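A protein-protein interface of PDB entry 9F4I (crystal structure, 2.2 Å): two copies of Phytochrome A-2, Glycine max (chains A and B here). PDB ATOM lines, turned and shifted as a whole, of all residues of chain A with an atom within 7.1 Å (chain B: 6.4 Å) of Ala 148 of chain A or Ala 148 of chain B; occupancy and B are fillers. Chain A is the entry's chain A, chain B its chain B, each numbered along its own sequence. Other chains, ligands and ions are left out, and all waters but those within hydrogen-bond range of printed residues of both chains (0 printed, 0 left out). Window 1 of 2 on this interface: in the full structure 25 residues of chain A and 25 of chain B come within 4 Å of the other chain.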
ATOM      1  N   TYR A 119       3.958  -2.103   7.094  1.00  0.00           N
ATOM      2  CA  TYR A 119       5.070  -1.204   6.805  1.00  0.00           C
ATOM      3  C   TYR A 119       6.203  -2.035   6.228  1.00  0.00           C
ATOM      4  O   TYR A 119       6.621  -3.022   6.849  1.00  0.00           O
ATOM      5  CB  TYR A 119       5.563  -0.498   8.060  1.00  0.00           C
ATOM      6  CG  TYR A 119       4.858   0.793   8.361  1.00  0.00           C
ATOM      7  CD1 TYR A 119       4.036   1.399   7.417  1.00  0.00           C
ATOM      8  CD2 TYR A 119       5.030   1.423   9.592  1.00  0.00           C
ATOM      9  CE1 TYR A 119       3.392   2.591   7.698  1.00  0.00           C
ATOM     10  CE2 TYR A 119       4.391   2.606   9.880  1.00  0.00           C
ATOM     11  CZ  TYR A 119       3.577   3.182   8.927  1.00  0.00           C
ATOM     12  OH  TYR A 119       2.938   4.360   9.217  1.00  0.00           O
ATOM     13  N   MET A 143      -4.952   6.408   9.666  1.00  0.00           N
ATOM     14  CA  MET A 143      -4.245   7.223  10.642  1.00  0.00           C
ATOM     15  C   MET A 143      -2.723   7.146  10.521  1.00  0.00           C
ATOM     16  O   MET A 143      -2.030   7.519  11.470  1.00  0.00           O
ATOM     17  CB  MET A 143      -4.652   6.790  12.051  1.00  0.00           C
ATOM     18  CG  MET A 143      -6.153   6.502  12.223  1.00  0.00           C
ATOM     19  SD  MET A 143      -7.207   7.799  11.528  1.00  0.00           S
ATOM     20  CE  MET A 143      -6.549   9.291  12.330  1.00  0.00           C
ATOM     21  N   THR A 144      -2.180   6.672   9.392  1.00  0.00           N
ATOM     22  CA  THR A 144      -0.735   6.441   9.319  1.00  0.00           C
ATOM     23  C   THR A 144       0.047   7.749   9.358  1.00  0.00           C
ATOM     24  O   THR A 144       0.933   7.936  10.205  1.00  0.00           O
ATOM     25  CB  THR A 144      -0.364   5.654   8.061  1.00  0.00           C
ATOM     26  OG1 THR A 144      -0.759   6.388   6.888  1.00  0.00           O
ATOM     27  CG2 THR A 144      -0.970   4.256   8.083  1.00  0.00           C
ATOM     28  N   ALA A 145      -0.262   8.665   8.437  1.00  0.00           N
ATOM     29  CA  ALA A 145       0.478   9.918   8.366  1.00  0.00           C
ATOM     30  C   ALA A 145       0.340  10.721   9.658  1.00  0.00           C
ATOM     31  O   ALA A 145       1.290  11.384  10.089  1.00  0.00           O
ATOM     32  CB  ALA A 145      -0.004  10.738   7.169  1.00  0.00           C
ATOM     33  N   ALA A 146      -0.834  10.668  10.298  1.00  0.00           N
ATOM     34  CA  ALA A 146      -1.032  11.438  11.524  1.00  0.00           C
ATOM     35  C   ALA A 146      -0.241  10.835  12.681  1.00  0.00           C
ATOM     36  O   ALA A 146       0.360  11.568  13.476  1.00  0.00           O
ATOM     37  CB  ALA A 146      -2.518  11.519  11.858  1.00  0.00           C
ATOM     38  N   GLY A 147      -0.194   9.501  12.772  1.00  0.00           N
ATOM     39  CA  GLY A 147       0.726   8.875  13.711  1.00  0.00           C
ATOM     40  C   GLY A 147       2.185   9.111  13.381  1.00  0.00           C
ATOM     41  O   GLY A 147       3.052   8.893  14.234  1.00  0.00           O
ATOM     42  N   ALA A 148       2.472   9.559  12.161  1.00  0.00           N
ATOM     43  CA  ALA A 148       3.839   9.862  11.758  1.00  0.00           C
ATOM     44  C   ALA A 148       4.204  11.312  12.064  1.00  0.00           C
ATOM     45  O   ALA A 148       5.294  11.602  12.579  1.00  0.00           O
ATOM     46  CB  ALA A 148       4.022   9.571  10.260  1.00  0.00           C
ATOM     47  N   LEU A 149       3.302  12.239  11.759  1.00  0.00           N
ATOM     48  CA  LEU A 149       3.509  13.622  12.169  1.00  0.00           C
ATOM     49  C   LEU A 149       3.460  13.755  13.687  1.00  0.00           C
ATOM     50  O   LEU A 149       4.184  14.559  14.273  1.00  0.00           O
ATOM     51  CB  LEU A 149       2.456  14.523  11.516  1.00  0.00           C
ATOM     52  CG  LEU A 149       2.263  14.339  10.008  1.00  0.00           C
ATOM     53  CD1 LEU A 149       0.927  14.951   9.627  1.00  0.00           C
ATOM     54  CD2 LEU A 149       3.400  14.948   9.184  1.00  0.00           C
ATOM     55  N   GLN A 150       2.607  12.984  14.345  1.00  0.00           N
ATOM     56  CA  GLN A 150       2.408  13.181  15.779  1.00  0.00           C
ATOM     57  C   GLN A 150       3.623  12.721  16.582  1.00  0.00           C
ATOM     58  O   GLN A 150       3.928  13.293  17.632  1.00  0.00           O
ATOM     59  CB  GLN A 150       1.136  12.451  16.224  1.00  0.00           C
ATOM     60  CG  GLN A 150       0.875  12.436  17.713  1.00  0.00           C
ATOM     61  CD  GLN A 150       0.580  13.813  18.288  1.00  0.00           C
ATOM     62  OE1 GLN A 150       0.408  14.807  17.560  1.00  0.00           O
ATOM     63  NE2 GLN A 150       0.523  13.877  19.615  1.00  0.00           N
ATOM     64  N   SER A 151       4.339  11.699  16.096  1.00  0.00           N
ATOM     65  CA  SER A 151       5.561  11.262  16.770  1.00  0.00           C
ATOM     66  C   SER A 151       6.706  12.245  16.538  1.00  0.00           C
ATOM     67  O   SER A 151       7.274  12.770  17.502  1.00  0.00           O
ATOM     68  CB  SER A 151       5.944   9.848  16.318  1.00  0.00           C
ATOM     69  OG  SER A 151       5.435   8.871  17.225  1.00  0.00           O
ATOM     70  N   TYR A 152       7.043  12.529  15.267  1.00  0.00           N
ATOM     71  CA  TYR A 152       8.148  13.447  14.944  1.00  0.00           C
ATOM     72  C   TYR A 152       7.937  14.841  15.526  1.00  0.00           C
ATOM     73  O   TYR A 152       8.902  15.595  15.692  1.00  0.00           O
ATOM     74  CB  TYR A 152       8.341  13.542  13.422  1.00  0.00           C
ATOM     75  CG  TYR A 152       9.774  13.727  12.924  1.00  0.00           C
ATOM     76  CD1 TYR A 152      10.575  14.751  13.396  1.00  0.00           C
ATOM     77  CD2 TYR A 152      10.309  12.876  11.958  1.00  0.00           C
ATOM     78  CE1 TYR A 152      11.876  14.921  12.924  1.00  0.00           C
ATOM     79  CE2 TYR A 152      11.608  13.038  11.488  1.00  0.00           C
ATOM     80  CZ  TYR A 152      12.386  14.064  11.971  1.00  0.00           C
ATOM     81  OH  TYR A 152      13.675  14.231  11.500  1.00  0.00           O
ATOM     82  N   LYS A 153       6.703  15.201  15.860  1.00  0.00           N
ATOM     83  CA  LYS A 153       6.461  16.531  16.414  1.00  0.00           C
ATOM     84  C   LYS A 153       6.781  16.578  17.905  1.00  0.00           C
ATOM     85  O   LYS A 153       7.141  17.634  18.447  1.00  0.00           O
ATOM     86  CB  LYS A 153       5.013  16.958  16.176  1.00  0.00           C
ATOM     87  CG  LYS A 153       4.677  18.327  16.765  1.00  0.00           C
ATOM     88  CD  LYS A 153       3.197  18.488  17.077  1.00  0.00           C
ATOM     89  CE  LYS A 153       2.872  19.967  17.327  1.00  0.00           C
ATOM     90  NZ  LYS A 153       1.421  20.221  17.608  1.00  0.00           N
ATOM     91  N   PRO A 331       7.673   4.686  12.634  1.00  0.00           N
ATOM     92  CA  PRO A 331       7.795   6.153  12.511  1.00  0.00           C
ATOM     93  C   PRO A 331       8.335   6.807  13.764  1.00  0.00           C
ATOM     94  O   PRO A 331       9.160   7.730  13.664  1.00  0.00           O
ATOM     95  CB  PRO A 331       6.358   6.603  12.200  1.00  0.00           C
ATOM     96  CG  PRO A 331       5.740   5.428  11.531  1.00  0.00           C
ATOM     97  CD  PRO A 331       6.310   4.235  12.274  1.00  0.00           C
ATOM     98  N   LEU A 332       7.914   6.341  14.939  1.00  0.00           N
ATOM     99  CA  LEU A 332       8.394   6.911  16.191  1.00  0.00           C
ATOM    100  C   LEU A 332       9.896   6.672  16.342  1.00  0.00           C
ATOM    101  O   LEU A 332      10.674   7.626  16.427  1.00  0.00           O
ATOM    102  CB  LEU A 332       7.627   6.318  17.369  1.00  0.00           C
ATOM    103  CG  LEU A 332       8.136   6.698  18.771  1.00  0.00           C
ATOM    104  CD1 LEU A 332       8.449   8.188  18.922  1.00  0.00           C
ATOM    105  CD2 LEU A 332       7.146   6.239  19.829  1.00  0.00           C
ATOM    106  N   ALA A 335      11.715   8.952  14.422  1.00  0.00           N
ATOM    107  CA  ALA A 335      11.828  10.298  14.981  1.00  0.00           C
ATOM    108  C   ALA A 335      12.837  10.346  16.129  1.00  0.00           C
ATOM    109  O   ALA A 335      13.554  11.336  16.292  1.00  0.00           O
ATOM    110  CB  ALA A 335      10.460  10.793  15.431  1.00  0.00           C
ATOM    111  N   TYR B 119      -6.677  13.106   1.400  1.00  0.00           N
ATOM    112  CA  TYR B 119      -6.414  13.498   2.787  1.00  0.00           C
ATOM    113  C   TYR B 119      -7.608  14.285   3.333  1.00  0.00           C
ATOM    114  O   TYR B 119      -8.103  15.219   2.685  1.00  0.00           O
ATOM    115  CB  TYR B 119      -5.149  14.356   2.902  1.00  0.00           C
ATOM    116  CG  TYR B 119      -3.841  13.607   2.880  1.00  0.00           C
ATOM    117  CD1 TYR B 119      -3.746  12.320   3.404  1.00  0.00           C
ATOM    118  CD2 TYR B 119      -2.684  14.193   2.378  1.00  0.00           C
ATOM    119  CE1 TYR B 119      -2.531  11.614   3.406  1.00  0.00           C
ATOM    120  CE2 TYR B 119      -1.453  13.474   2.366  1.00  0.00           C
ATOM    121  CZ  TYR B 119      -1.405  12.194   2.897  1.00  0.00           C
ATOM    122  OH  TYR B 119      -0.230  11.499   2.893  1.00  0.00           O
ATOM    123  N   MET B 143       3.365   5.793  -0.133  1.00  0.00           N
ATOM    124  CA  MET B 143       4.422   6.694   0.352  1.00  0.00           C
ATOM    125  C   MET B 143       3.961   7.698   1.414  1.00  0.00           C
ATOM    126  O   MET B 143       4.703   8.640   1.734  1.00  0.00           O
ATOM    127  CB  MET B 143       5.003   7.525  -0.804  1.00  0.00           C
ATOM    128  CG  MET B 143       5.341   6.782  -2.021  1.00  0.00           C
ATOM    129  SD  MET B 143       6.237   5.279  -1.627  1.00  0.00           S
ATOM    130  CE  MET B 143       7.772   5.963  -0.970  1.00  0.00           C
ATOM    131  N   THR B 144       2.753   7.556   1.949  1.00  0.00           N
ATOM    132  CA  THR B 144       2.246   8.638   2.783  1.00  0.00           C
ATOM    133  C   THR B 144       2.879   8.693   4.158  1.00  0.00           C
ATOM    134  O   THR B 144       2.799   9.730   4.818  1.00  0.00           O
ATOM    135  CB  THR B 144       0.738   8.530   2.899  1.00  0.00           C
ATOM    136  OG1 THR B 144       0.368   7.222   3.322  1.00  0.00           O
ATOM    137  CG2 THR B 144       0.140   8.829   1.505  1.00  0.00           C
ATOM    138  N   ALA B 145       3.510   7.626   4.624  1.00  0.00           N
ATOM    139  CA  ALA B 145       4.043   7.708   5.979  1.00  0.00           C
ATOM    140  C   ALA B 145       5.426   8.344   5.989  1.00  0.00           C
ATOM    141  O   ALA B 145       5.766   9.130   6.891  1.00  0.00           O
ATOM    142  CB  ALA B 145       4.035   6.310   6.595  1.00  0.00           C
ATOM    143  N   ALA B 146       6.182   8.076   4.944  1.00  0.00           N
ATOM    144  CA  ALA B 146       7.551   8.500   4.769  1.00  0.00           C
ATOM    145  C   ALA B 146       7.675   9.826   4.021  1.00  0.00           C
ATOM    146  O   ALA B 146       8.792  10.336   3.864  1.00  0.00           O
ATOM    147  CB  ALA B 146       8.291   7.422   3.992  1.00  0.00           C
ATOM    148  N   GLY B 147       6.565  10.384   3.551  1.00  0.00           N
ATOM    149  CA  GLY B 147       6.551  11.747   3.060  1.00  0.00           C
ATOM    150  C   GLY B 147       6.301  12.641   4.255  1.00  0.00           C
ATOM    151  O   GLY B 147       6.976  13.662   4.462  1.00  0.00           O
ATOM    152  N   ALA B 148       5.326  12.247   5.069  1.00  0.00           N
ATOM    153  CA  ALA B 148       5.196  12.809   6.414  1.00  0.00           C
ATOM    154  C   ALA B 148       6.548  12.898   7.135  1.00  0.00           C
ATOM    155  O   ALA B 148       6.948  13.976   7.600  1.00  0.00           O
ATOM    156  CB  ALA B 148       4.214  11.960   7.232  1.00  0.00           C
ATOM    157  N   LEU B 149       7.265  11.771   7.245  1.00  0.00           N
ATOM    158  CA  LEU B 149       8.482  11.733   8.062  1.00  0.00           C
ATOM    159  C   LEU B 149       9.561  12.649   7.510  1.00  0.00           C
ATOM    160  O   LEU B 149      10.240  13.351   8.270  1.00  0.00           O
ATOM    161  CB  LEU B 149       9.024  10.304   8.144  1.00  0.00           C
ATOM    162  CG  LEU B 149       8.353   9.448   9.227  1.00  0.00           C
ATOM    163  CD1 LEU B 149       8.955   8.032   9.071  1.00  0.00           C
ATOM    164  CD2 LEU B 149       8.595  10.003  10.615  1.00  0.00           C
ATOM    165  N   GLN B 150       9.763  12.613   6.193  1.00  0.00           N
ATOM    166  CA  GLN B 150      10.762  13.455   5.554  1.00  0.00           C
ATOM    167  C   GLN B 150      10.428  14.935   5.730  1.00  0.00           C
ATOM    168  O   GLN B 150      11.296  15.742   6.096  1.00  0.00           O
ATOM    169  CB  GLN B 150      10.837  13.095   4.073  1.00  0.00           C
ATOM    170  CG  GLN B 150      11.850  13.907   3.283  1.00  0.00           C
ATOM    171  CD  GLN B 150      13.214  13.256   3.307  1.00  0.00           C
ATOM    172  OE1 GLN B 150      13.543  12.499   4.234  1.00  0.00           O
ATOM    173  NE2 GLN B 150      14.013  13.524   2.276  1.00  0.00           N
ATOM    174  N   SER B 151       9.157  15.300   5.496  1.00  0.00           N
ATOM    175  CA  SER B 151       8.715  16.682   5.654  1.00  0.00           C
ATOM    176  C   SER B 151       9.126  17.231   7.011  1.00  0.00           C
ATOM    177  O   SER B 151       9.757  18.285   7.101  1.00  0.00           O
ATOM    178  CB  SER B 151       7.192  16.775   5.481  1.00  0.00           C
ATOM    179  OG  SER B 151       6.800  16.278   4.217  1.00  0.00           O
ATOM    180  N   TYR B 152       8.781  16.522   8.089  1.00  0.00           N
ATOM    181  CA  TYR B 152       9.211  16.975   9.403  1.00  0.00           C
ATOM    182  C   TYR B 152      10.721  16.903   9.557  1.00  0.00           C
ATOM    183  O   TYR B 152      11.304  17.701  10.296  1.00  0.00           O
ATOM    184  CB  TYR B 152       8.545  16.153  10.499  1.00  0.00           C
ATOM    185  CG  TYR B 152       7.826  17.032  11.495  1.00  0.00           C
ATOM    186  CD1 TYR B 152       8.415  17.415  12.701  1.00  0.00           C
ATOM    187  CD2 TYR B 152       6.563  17.509  11.207  1.00  0.00           C
ATOM    188  CE1 TYR B 152       7.728  18.244  13.598  1.00  0.00           C
ATOM    189  CE2 TYR B 152       5.872  18.323  12.079  1.00  0.00           C
ATOM    190  CZ  TYR B 152       6.447  18.687  13.261  1.00  0.00           C
ATOM    191  OH  TYR B 152       5.706  19.507  14.062  1.00  0.00           O
ATOM    192  N   LYS B 153      11.371  15.956   8.885  1.00  0.00           N
ATOM    193  CA  LYS B 153      12.807  15.820   9.055  1.00  0.00           C
ATOM    194  C   LYS B 153      13.547  17.068   8.566  1.00  0.00           C
ATOM    195  O   LYS B 153      14.525  17.507   9.191  1.00  0.00           O
ATOM    196  CB  LYS B 153      13.304  14.561   8.332  1.00  0.00           C
ATOM    197  CG  LYS B 153      14.818  14.351   8.550  1.00  0.00           C
ATOM    198  CD  LYS B 153      15.435  13.171   7.822  1.00  0.00           C
ATOM    199  CE  LYS B 153      16.702  12.702   8.597  1.00  0.00           C
ATOM    200  NZ  LYS B 153      17.319  11.408   8.128  1.00  0.00           N
ATOM    201  N   PRO B 331       1.109  17.432   4.911  1.00  0.00           N
ATOM    202  CA  PRO B 331       2.249  17.134   5.815  1.00  0.00           C
ATOM    203  C   PRO B 331       3.281  18.247   5.863  1.00  0.00           C
ATOM    204  O   PRO B 331       3.786  18.574   6.955  1.00  0.00           O
ATOM    205  CB  PRO B 331       2.831  15.827   5.246  1.00  0.00           C
ATOM    206  CG  PRO B 331       1.714  15.200   4.529  1.00  0.00           C
ATOM    207  CD  PRO B 331       0.867  16.327   3.954  1.00  0.00           C
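Among the printed residues, merely in contact across the chains: Tyr 152 of chain A with Lys 153 of chain B, Lys 153 of chain A with Tyr 152 of chain B, Tyr 119 of chain A with Ala 145 of chain B, Tyr 152 of chain A with Tyr 152 of chain B, Tyr 152 of chain A with Leu 149 of chain B, Leu 149 of chain A with Ala 148 of chain B, Ala 145 of chain A with Thr 144 of chain B, Ala 148 of chain A with Ala 145 of chain B, Thr 144 of chain A with Thr 144 of chain B, Pro 331 of chain A with Leu 149 of chain B and Ala 148 of chain A with Ala 148 of chain B.
Met 143 of chain A touches none of the printed residues of chain B. Ala 148 of chain A touches just these residues of chain B: Ala 145 and Ala 148. Of the printed residues of chain B, Leu 149 of chain A touches Ala 148. Printed residues of chain B within 4 Å of Pro 331 of chain A: Leu 149. Leu 332 of chain A touches none of the printed residues of chain B. Gly 147 of chain B touches none of the printed residues of chain A. Of the printed residues of chain A, Ala 148 of chain B touches Ala 148 (3.9 Å) and Leu 149 (3.7 Å). Of the printed residues of chain A, Lys 153 of chain B touches Tyr 152 (3.0 Å). The nearest residue of chain B that does not touch Ala 148 of chain A is Leu 149 of chain B (4.2 Å).
Ala 145 of chain A touches Thr 144 of chain B, but with the chains exchanged Thr 144 of chain A does not touch Ala 145 of chain B (4.7 Å). Ala 148 of chain B touches its own counterpart, Ala 148 of chain A. Tyr 152 of chain A touches Lys 153 of chain B, and with the chains exchanged Lys 153 of chain A touches Tyr 152 of chain B. Pro 331 of chain A touches Leu 149 of chain B, but with the chains exchanged Leu 149 of chain A does not touch Pro 331 of chain B (4.1 Å). Positions printed for both chains: 119, 143, 144, 145, 146, 147, 148, 149, 150, 151, 152, 153 and 331. Of the 11 pairs that touch across the chains among the printed residues, 5 have their exchanged pair printed and touching as well.
Of the 15 printed residues of chain A, 8 touch a printed residue of chain B. Along chain A the printed residues that touch a printed residue of chain B span positions 119 to 331. Hydrophobic or aromatic side chains of chain B that line the printed part of chain A: Ala 145, Ala 148, Leu 149 and Tyr 152. Among the printed residues, no Asp or Glu carboxylate lies within 4 Å of a Lys or Arg side-chain nitrogen of the other chain.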
